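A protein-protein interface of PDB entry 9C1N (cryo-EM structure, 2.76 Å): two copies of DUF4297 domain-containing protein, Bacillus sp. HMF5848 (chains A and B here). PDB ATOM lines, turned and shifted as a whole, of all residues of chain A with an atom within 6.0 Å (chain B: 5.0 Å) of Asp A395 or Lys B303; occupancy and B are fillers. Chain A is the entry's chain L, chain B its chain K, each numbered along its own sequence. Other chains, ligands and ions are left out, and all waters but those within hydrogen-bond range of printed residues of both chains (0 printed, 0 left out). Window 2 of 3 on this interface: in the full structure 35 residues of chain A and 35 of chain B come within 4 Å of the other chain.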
ATOM      1  N   SER A 279      15.303  12.494 -25.337  1.00  0.00           N
ATOM      2  CA  SER A 279      16.658  12.065 -25.677  1.00  0.00           C
ATOM      3  C   SER A 279      17.432  11.623 -24.438  1.00  0.00           C
ATOM      4  O   SER A 279      18.567  12.046 -24.204  1.00  0.00           O
ATOM      5  CB  SER A 279      17.408  13.174 -26.410  1.00  0.00           C
ATOM      6  OG  SER A 279      17.568  14.314 -25.584  1.00  0.00           O
ATOM      7  N   ARG A 280      16.830  10.761 -23.625  1.00  0.00           N
ATOM      8  CA  ARG A 280      17.530  10.142 -22.509  1.00  0.00           C
ATOM      9  C   ARG A 280      17.893   8.700 -22.843  1.00  0.00           C
ATOM     10  O   ARG A 280      17.150   7.994 -23.530  1.00  0.00           O
ATOM     11  CB  ARG A 280      16.691  10.171 -21.231  1.00  0.00           C
ATOM     12  CG  ARG A 280      16.010  11.492 -20.960  1.00  0.00           C
ATOM     13  CD  ARG A 280      15.652  11.641 -19.488  1.00  0.00           C
ATOM     14  NE  ARG A 280      16.771  11.344 -18.601  1.00  0.00           N
ATOM     15  CZ  ARG A 280      17.385  12.246 -17.847  1.00  0.00           C
ATOM     16  NH1 ARG A 280      17.027  13.518 -17.863  1.00  0.00           N
ATOM     17  NH2 ARG A 280      18.383  11.861 -17.058  1.00  0.00           N
ATOM     18  N   SER A 281      19.050   8.272 -22.347  1.00  0.00           N
ATOM     19  CA  SER A 281      19.495   6.893 -22.486  1.00  0.00           C
ATOM     20  C   SER A 281      19.003   6.095 -21.285  1.00  0.00           C
ATOM     21  O   SER A 281      19.397   6.372 -20.147  1.00  0.00           O
ATOM     22  CB  SER A 281      21.018   6.822 -22.600  1.00  0.00           C
ATOM     23  OG  SER A 281      21.638   7.242 -21.398  1.00  0.00           O
ATOM     24  N   ARG A 282      18.146   5.109 -21.537  1.00  0.00           N
ATOM     25  CA  ARG A 282      17.519   4.322 -20.487  1.00  0.00           C
ATOM     26  C   ARG A 282      17.967   2.873 -20.599  1.00  0.00           C
ATOM     27  O   ARG A 282      17.876   2.272 -21.675  1.00  0.00           O
ATOM     28  CB  ARG A 282      15.993   4.413 -20.570  1.00  0.00           C
ATOM     29  CG  ARG A 282      15.472   5.838 -20.672  1.00  0.00           C
ATOM     30  CD  ARG A 282      13.953   5.879 -20.636  1.00  0.00           C
ATOM     31  NE  ARG A 282      13.440   7.195 -20.993  1.00  0.00           N
ATOM     32  CZ  ARG A 282      13.242   7.609 -22.238  1.00  0.00           C
ATOM     33  NH1 ARG A 282      13.506   6.832 -23.275  1.00  0.00           N
ATOM     34  NH2 ARG A 282      12.770   8.834 -22.447  1.00  0.00           N
ATOM     35  N   GLU A 318      18.525   8.377 -28.666  1.00  0.00           N
ATOM     36  CA  GLU A 318      19.198   7.362 -27.871  1.00  0.00           C
ATOM     37  C   GLU A 318      18.516   6.007 -28.032  1.00  0.00           C
ATOM     38  O   GLU A 318      17.318   5.921 -28.312  1.00  0.00           O
ATOM     39  CB  GLU A 318      19.230   7.764 -26.396  1.00  0.00           C
ATOM     40  CG  GLU A 318      20.100   8.978 -26.105  1.00  0.00           C
ATOM     41  CD  GLU A 318      21.521   8.820 -26.617  1.00  0.00           C
ATOM     42  OE1 GLU A 318      22.082   7.711 -26.498  1.00  0.00           O
ATOM     43  OE2 GLU A 318      22.076   9.808 -27.144  1.00  0.00           O
ATOM     44  N   LYS A 393      28.042   5.202 -19.450  1.00  0.00           N
ATOM     45  CA  LYS A 393      27.019   5.335 -18.423  1.00  0.00           C
ATOM     46  C   LYS A 393      25.718   5.872 -19.007  1.00  0.00           C
ATOM     47  O   LYS A 393      25.703   6.566 -20.028  1.00  0.00           O
ATOM     48  CB  LYS A 393      27.502   6.253 -17.302  1.00  0.00           C
ATOM     49  CG  LYS A 393      28.231   5.532 -16.189  1.00  0.00           C
ATOM     50  CD  LYS A 393      29.076   6.497 -15.380  1.00  0.00           C
ATOM     51  CE  LYS A 393      29.073   6.107 -13.917  1.00  0.00           C
ATOM     52  NZ  LYS A 393      29.955   6.986 -13.102  1.00  0.00           N
ATOM     53  N   CYS A 394      24.620   5.544 -18.337  1.00  0.00           N
ATOM     54  CA  CYS A 394      23.285   5.934 -18.759  1.00  0.00           C
ATOM     55  C   CYS A 394      22.767   7.086 -17.904  1.00  0.00           C
ATOM     56  O   CYS A 394      23.380   7.493 -16.914  1.00  0.00           O
ATOM     57  CB  CYS A 394      22.328   4.741 -18.679  1.00  0.00           C
ATOM     58  SG  CYS A 394      22.306   3.926 -17.065  1.00  0.00           S
ATOM     59  N   ASP A 395      21.614   7.616 -18.309  1.00  0.00           N
ATOM     60  CA  ASP A 395      20.933   8.653 -17.545  1.00  0.00           C
ATOM     61  C   ASP A 395      19.972   8.064 -16.519  1.00  0.00           C
ATOM     62  O   ASP A 395      19.829   8.607 -15.418  1.00  0.00           O
ATOM     63  CB  ASP A 395      20.183   9.593 -18.491  1.00  0.00           C
ATOM     64  CG  ASP A 395      21.119  10.438 -19.331  1.00  0.00           C
ATOM     65  OD1 ASP A 395      22.238  10.735 -18.863  1.00  0.00           O
ATOM     66  OD2 ASP A 395      20.738  10.805 -20.463  1.00  0.00           O
ATOM     67  N   ASP A 396      19.310   6.960 -16.865  1.00  0.00           N
ATOM     68  CA  ASP A 396      18.436   6.238 -15.954  1.00  0.00           C
ATOM     69  C   ASP A 396      18.782   4.757 -16.008  1.00  0.00           C
ATOM     70  O   ASP A 396      19.063   4.216 -17.080  1.00  0.00           O
ATOM     71  CB  ASP A 396      16.959   6.444 -16.308  1.00  0.00           C
ATOM     72  CG  ASP A 396      16.504   7.877 -16.106  1.00  0.00           C
ATOM     73  OD1 ASP A 396      16.131   8.229 -14.968  1.00  0.00           O
ATOM     74  OD2 ASP A 396      16.521   8.652 -17.086  1.00  0.00           O
ATOM     75  N   LEU A 397      18.758   4.104 -14.845  1.00  0.00           N
ATOM     76  CA  LEU A 397      19.062   2.678 -14.729  1.00  0.00           C
ATOM     77  C   LEU A 397      17.903   2.013 -13.992  1.00  0.00           C
ATOM     78  O   LEU A 397      17.911   1.910 -12.762  1.00  0.00           O
ATOM     79  CB  LEU A 397      20.393   2.453 -14.020  1.00  0.00           C
ATOM     80  CG  LEU A 397      20.861   1.000 -13.916  1.00  0.00           C
ATOM     81  CD1 LEU A 397      21.124   0.421 -15.295  1.00  0.00           C
ATOM     82  CD2 LEU A 397      22.099   0.894 -13.040  1.00  0.00           C
ATOM     83  N   ASP A 412      26.732   8.529  -9.572  1.00  0.00           N
ATOM     84  CA  ASP A 412      26.140   9.603 -10.370  1.00  0.00           C
ATOM     85  C   ASP A 412      25.233   9.063 -11.474  1.00  0.00           C
ATOM     86  O   ASP A 412      25.203   9.585 -12.590  1.00  0.00           O
ATOM     87  CB  ASP A 412      27.222  10.514 -10.956  1.00  0.00           C
ATOM     88  CG  ASP A 412      27.927  11.334  -9.896  1.00  0.00           C
ATOM     89  OD1 ASP A 412      27.296  11.644  -8.865  1.00  0.00           O
ATOM     90  OD2 ASP A 412      29.116  11.666 -10.093  1.00  0.00           O
ATOM     91  N   VAL A 413      24.483   8.008 -11.164  1.00  0.00           N
ATOM     92  CA  VAL A 413      23.451   7.501 -12.058  1.00  0.00           C
ATOM     93  C   VAL A 413      22.139   7.451 -11.289  1.00  0.00           C
ATOM     94  O   VAL A 413      22.116   7.252 -10.070  1.00  0.00           O
ATOM     95  CB  VAL A 413      23.794   6.111 -12.642  1.00  0.00           C
ATOM     96  CG1 VAL A 413      25.064   6.180 -13.480  1.00  0.00           C
ATOM     97  CG2 VAL A 413      23.918   5.076 -11.539  1.00  0.00           C
ATOM     98  N   ASN A 414      21.039   7.645 -12.011  1.00  0.00           N
ATOM     99  CA  ASN A 414      19.708   7.641 -11.414  1.00  0.00           C
ATOM    100  C   ASN A 414      19.181   6.211 -11.418  1.00  0.00           C
ATOM    101  O   ASN A 414      18.784   5.690 -12.465  1.00  0.00           O
ATOM    102  CB  ASN A 414      18.773   8.580 -12.171  1.00  0.00           C
ATOM    103  CG  ASN A 414      17.616   9.060 -11.319  1.00  0.00           C
ATOM    104  OD1 ASN A 414      17.799   9.442 -10.162  1.00  0.00           O
ATOM    105  ND2 ASN A 414      16.415   9.045 -11.885  1.00  0.00           N
ATOM    106  N   ILE B 299      25.687  16.203  -8.092  1.00  0.00           N
ATOM    107  CA  ILE B 299      25.871  16.113  -9.538  1.00  0.00           C
ATOM    108  C   ILE B 299      24.534  15.895 -10.237  1.00  0.00           C
ATOM    109  O   ILE B 299      24.248  16.517 -11.268  1.00  0.00           O
ATOM    110  CB  ILE B 299      26.875  14.997  -9.879  1.00  0.00           C
ATOM    111  CG1 ILE B 299      28.089  15.059  -8.948  1.00  0.00           C
ATOM    112  CG2 ILE B 299      27.312  15.096 -11.330  1.00  0.00           C
ATOM    113  CD1 ILE B 299      28.876  16.342  -9.043  1.00  0.00           C
ATOM    114  N   LEU B 300      23.697  15.008  -9.692  1.00  0.00           N
ATOM    115  CA  LEU B 300      22.414  14.709 -10.319  1.00  0.00           C
ATOM    116  C   LEU B 300      21.477  15.910 -10.269  1.00  0.00           C
ATOM    117  O   LEU B 300      20.717  16.151 -11.215  1.00  0.00           O
ATOM    118  CB  LEU B 300      21.774  13.497  -9.642  1.00  0.00           C
ATOM    119  CG  LEU B 300      22.511  12.170  -9.844  1.00  0.00           C
ATOM    120  CD1 LEU B 300      21.969  11.103  -8.906  1.00  0.00           C
ATOM    121  CD2 LEU B 300      22.415  11.719 -11.293  1.00  0.00           C
ATOM    122  N   PHE B 301      21.507  16.668  -9.170  1.00  0.00           N
ATOM    123  CA  PHE B 301      20.691  17.875  -9.075  1.00  0.00           C
ATOM    124  C   PHE B 301      21.067  18.876 -10.160  1.00  0.00           C
ATOM    125  O   PHE B 301      20.195  19.436 -10.835  1.00  0.00           O
ATOM    126  CB  PHE B 301      20.842  18.500  -7.687  1.00  0.00           C
ATOM    127  CG  PHE B 301      20.366  19.923  -7.606  1.00  0.00           C
ATOM    128  CD1 PHE B 301      19.020  20.211  -7.472  1.00  0.00           C
ATOM    129  CD2 PHE B 301      21.268  20.975  -7.659  1.00  0.00           C
ATOM    130  CE1 PHE B 301      18.584  21.519  -7.397  1.00  0.00           C
ATOM    131  CE2 PHE B 301      20.834  22.283  -7.587  1.00  0.00           C
ATOM    132  CZ  PHE B 301      19.491  22.554  -7.455  1.00  0.00           C
ATOM    133  N   VAL B 302      22.368  19.107 -10.343  1.00  0.00           N
ATOM    134  CA  VAL B 302      22.822  20.032 -11.375  1.00  0.00           C
ATOM    135  C   VAL B 302      22.466  19.503 -12.758  1.00  0.00           C
ATOM    136  O   VAL B 302      22.084  20.269 -13.650  1.00  0.00           O
ATOM    137  CB  VAL B 302      24.333  20.290 -11.234  1.00  0.00           C
ATOM    138  CG1 VAL B 302      24.848  21.131 -12.396  1.00  0.00           C
ATOM    139  CG2 VAL B 302      24.633  20.969  -9.911  1.00  0.00           C
ATOM    140  N   LYS B 303      22.579  18.189 -12.959  1.00  0.00           N
ATOM    141  CA  LYS B 303      22.223  17.606 -14.249  1.00  0.00           C
ATOM    142  C   LYS B 303      20.750  17.842 -14.571  1.00  0.00           C
ATOM    143  O   LYS B 303      20.406  18.260 -15.681  1.00  0.00           O
ATOM    144  CB  LYS B 303      22.546  16.112 -14.254  1.00  0.00           C
ATOM    145  CG  LYS B 303      22.511  15.475 -15.634  1.00  0.00           C
ATOM    146  CD  LYS B 303      22.862  13.997 -15.569  1.00  0.00           C
ATOM    147  CE  LYS B 303      22.786  13.355 -16.944  1.00  0.00           C
ATOM    148  NZ  LYS B 303      21.421  13.459 -17.527  1.00  0.00           N
ATOM    149  N   ASP B 304      19.866  17.589 -13.603  1.00  0.00           N
ATOM    150  CA  ASP B 304      18.441  17.815 -13.829  1.00  0.00           C
ATOM    151  C   ASP B 304      18.146  19.293 -14.058  1.00  0.00           C
ATOM    152  O   ASP B 304      17.332  19.649 -14.923  1.00  0.00           O
ATOM    153  CB  ASP B 304      17.630  17.280 -12.649  1.00  0.00           C
ATOM    154  CG  ASP B 304      17.656  15.766 -12.563  1.00  0.00           C
ATOM    155  OD1 ASP B 304      17.789  15.113 -13.619  1.00  0.00           O
ATOM    156  OD2 ASP B 304      17.541  15.229 -11.442  1.00  0.00           O
ATOM    157  N   TYR B 305      18.806  20.171 -13.297  1.00  0.00           N
ATOM    158  CA  TYR B 305      18.607  21.604 -13.481  1.00  0.00           C
ATOM    159  C   TYR B 305      19.029  22.040 -14.880  1.00  0.00           C
ATOM    160  O   TYR B 305      18.373  22.885 -15.497  1.00  0.00           O
ATOM    161  CB  TYR B 305      19.376  22.381 -12.409  1.00  0.00           C
ATOM    162  CG  TYR B 305      19.219  23.887 -12.490  1.00  0.00           C
ATOM    163  CD1 TYR B 305      19.997  24.645 -13.356  1.00  0.00           C
ATOM    164  CD2 TYR B 305      18.288  24.549 -11.701  1.00  0.00           C
ATOM    165  CE1 TYR B 305      19.852  26.017 -13.432  1.00  0.00           C
ATOM    166  CE2 TYR B 305      18.138  25.922 -11.771  1.00  0.00           C
ATOM    167  CZ  TYR B 305      18.923  26.650 -12.639  1.00  0.00           C
ATOM    168  OH  TYR B 305      18.779  28.016 -12.712  1.00  0.00           O
ATOM    169  N   LEU B 306      20.128  21.481 -15.394  1.00  0.00           N
ATOM    170  CA  LEU B 306      20.569  21.832 -16.740  1.00  0.00           C
ATOM    171  C   LEU B 306      19.632  21.267 -17.800  1.00  0.00           C
ATOM    172  O   LEU B 306      19.328  21.945 -18.789  1.00  0.00           O
ATOM    173  CB  LEU B 306      22.002  21.351 -16.971  1.00  0.00           C
ATOM    174  CG  LEU B 306      23.075  22.010 -16.102  1.00  0.00           C
ATOM    175  CD1 LEU B 306      24.464  21.555 -16.522  1.00  0.00           C
ATOM    176  CD2 LEU B 306      22.961  23.525 -16.157  1.00  0.00           C
ATOM    177  N   ASP B 307      19.164  20.029 -17.622  1.00  0.00           N
ATOM    178  CA  ASP B 307      18.206  19.472 -18.574  1.00  0.00           C
ATOM    179  C   ASP B 307      16.876  20.215 -18.576  1.00  0.00           C
ATOM    180  O   ASP B 307      16.162  20.170 -19.583  1.00  0.00           O
ATOM    181  CB  ASP B 307      17.962  17.982 -18.311  1.00  0.00           C
ATOM    182  CG  ASP B 307      19.144  17.113 -18.705  1.00  0.00           C
ATOM    183  OD1 ASP B 307      20.066  16.925 -17.891  1.00  0.00           O
ATOM    184  OD2 ASP B 307      19.146  16.610 -19.848  1.00  0.00           O
ATOM    185  N   ARG B 341      31.048  12.833 -16.121  1.00  0.00           N
ATOM    186  CA  ARG B 341      29.673  12.659 -16.571  1.00  0.00           C
ATOM    187  C   ARG B 341      29.345  13.497 -17.804  1.00  0.00           C
ATOM    188  O   ARG B 341      28.165  13.709 -18.105  1.00  0.00           O
ATOM    189  CB  ARG B 341      28.702  12.983 -15.435  1.00  0.00           C
ATOM    190  CG  ARG B 341      28.641  11.918 -14.353  1.00  0.00           C
ATOM    191  CD  ARG B 341      27.935  10.670 -14.861  1.00  0.00           C
ATOM    192  NE  ARG B 341      26.521  10.915 -15.124  1.00  0.00           N
ATOM    193  CZ  ARG B 341      25.792  10.231 -15.996  1.00  0.00           C
ATOM    194  NH1 ARG B 341      26.316   9.255 -16.719  1.00  0.00           N
ATOM    195  NH2 ARG B 341      24.508  10.538 -16.150  1.00  0.00           N
ATOM    196  N   ILE B 343      29.665  16.712 -18.377  1.00  0.00           N
ATOM    197  CA  ILE B 343      29.081  18.009 -18.053  1.00  0.00           C
ATOM    198  C   ILE B 343      30.210  19.026 -18.000  1.00  0.00           C
ATOM    199  O   ILE B 343      31.194  18.829 -17.279  1.00  0.00           O
ATOM    200  CB  ILE B 343      28.305  17.976 -16.724  1.00  0.00           C
ATOM    201  CG1 ILE B 343      27.194  16.924 -16.778  1.00  0.00           C
ATOM    202  CG2 ILE B 343      27.726  19.346 -16.411  1.00  0.00           C
ATOM    203  CD1 ILE B 343      26.423  16.777 -15.484  1.00  0.00           C
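NZ of Lys B303 is in salt-bridge range of OD1 of Asp A395, at 3.1 Å.
The guanidinium group of Arg B341 sits at hydrogen-bond distance from the backbone carbonyl oxygen of Cys A394 (3.3 Å).
The guanidinium group (NH2) of Arg B341 is in salt-bridge range of the side-chain carboxylate (OD1) of Asp A395.
The side-chain amino group of Lys B303 sits close to the guanidinium group of Arg A280 (3.5 Å).
The backbone carbonyl oxygen (O) of Asp A412 lies within hydrogen-bond range of the guanidinium group (NE) of Arg B341 (3.2 Å).
The backbone carbonyl oxygen (O) of Asp A396 is in hydrogen-bond range of the side-chain sulfur (SG) of Cys A394 (3.3 Å).
The side-chain hydroxyl (OG) of Ser A281 sits at hydrogen-bond distance from the backbone NH (N) of Asp A395, at 3.1 Å.
NZ of Lys B303 is in salt-bridge range of OD1 of Asp B307 (3.7 Å).
The side-chain carboxylate (OD2) of Asp A396 lies within salt-bridge range of the guanidinium group (NE) of Arg A280 (3.1 Å).
Among the printed residues, merely in contact across the chains: Lys A393 with Arg B341 (3.3 Å), Asp A412 with Ile B299 (3.5 Å) and Asp A412 with Leu B300 (3.7 Å).
Asp A395 touches just these residues of chain B: Lys B303 (3.1 Å) and Arg B341 (3.5 Å).
Lys B303 touches two residues of chain A.
Of the printed residues of chain A, Leu B300 touches Asp A412 (3.7 Å).
Of the printed residues of chain B, Cys A394 touches Arg B341.
The nearest printed residue of chain A that does not touch Ile B299 is Val A413 (7.5 Å).
Printed residues of chain B that touch a printed residue of chain A: Ile B299, Leu B300, Lys B303 and Arg B341.
Along chain B the printed residues that touch a printed residue of chain A span positions 299 to 341.
Printed residues of chain A that touch a printed residue of chain B: Arg A280, Lys A393, Cys A394, Asp A395 and Asp A412.
No position is printed for both chains.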
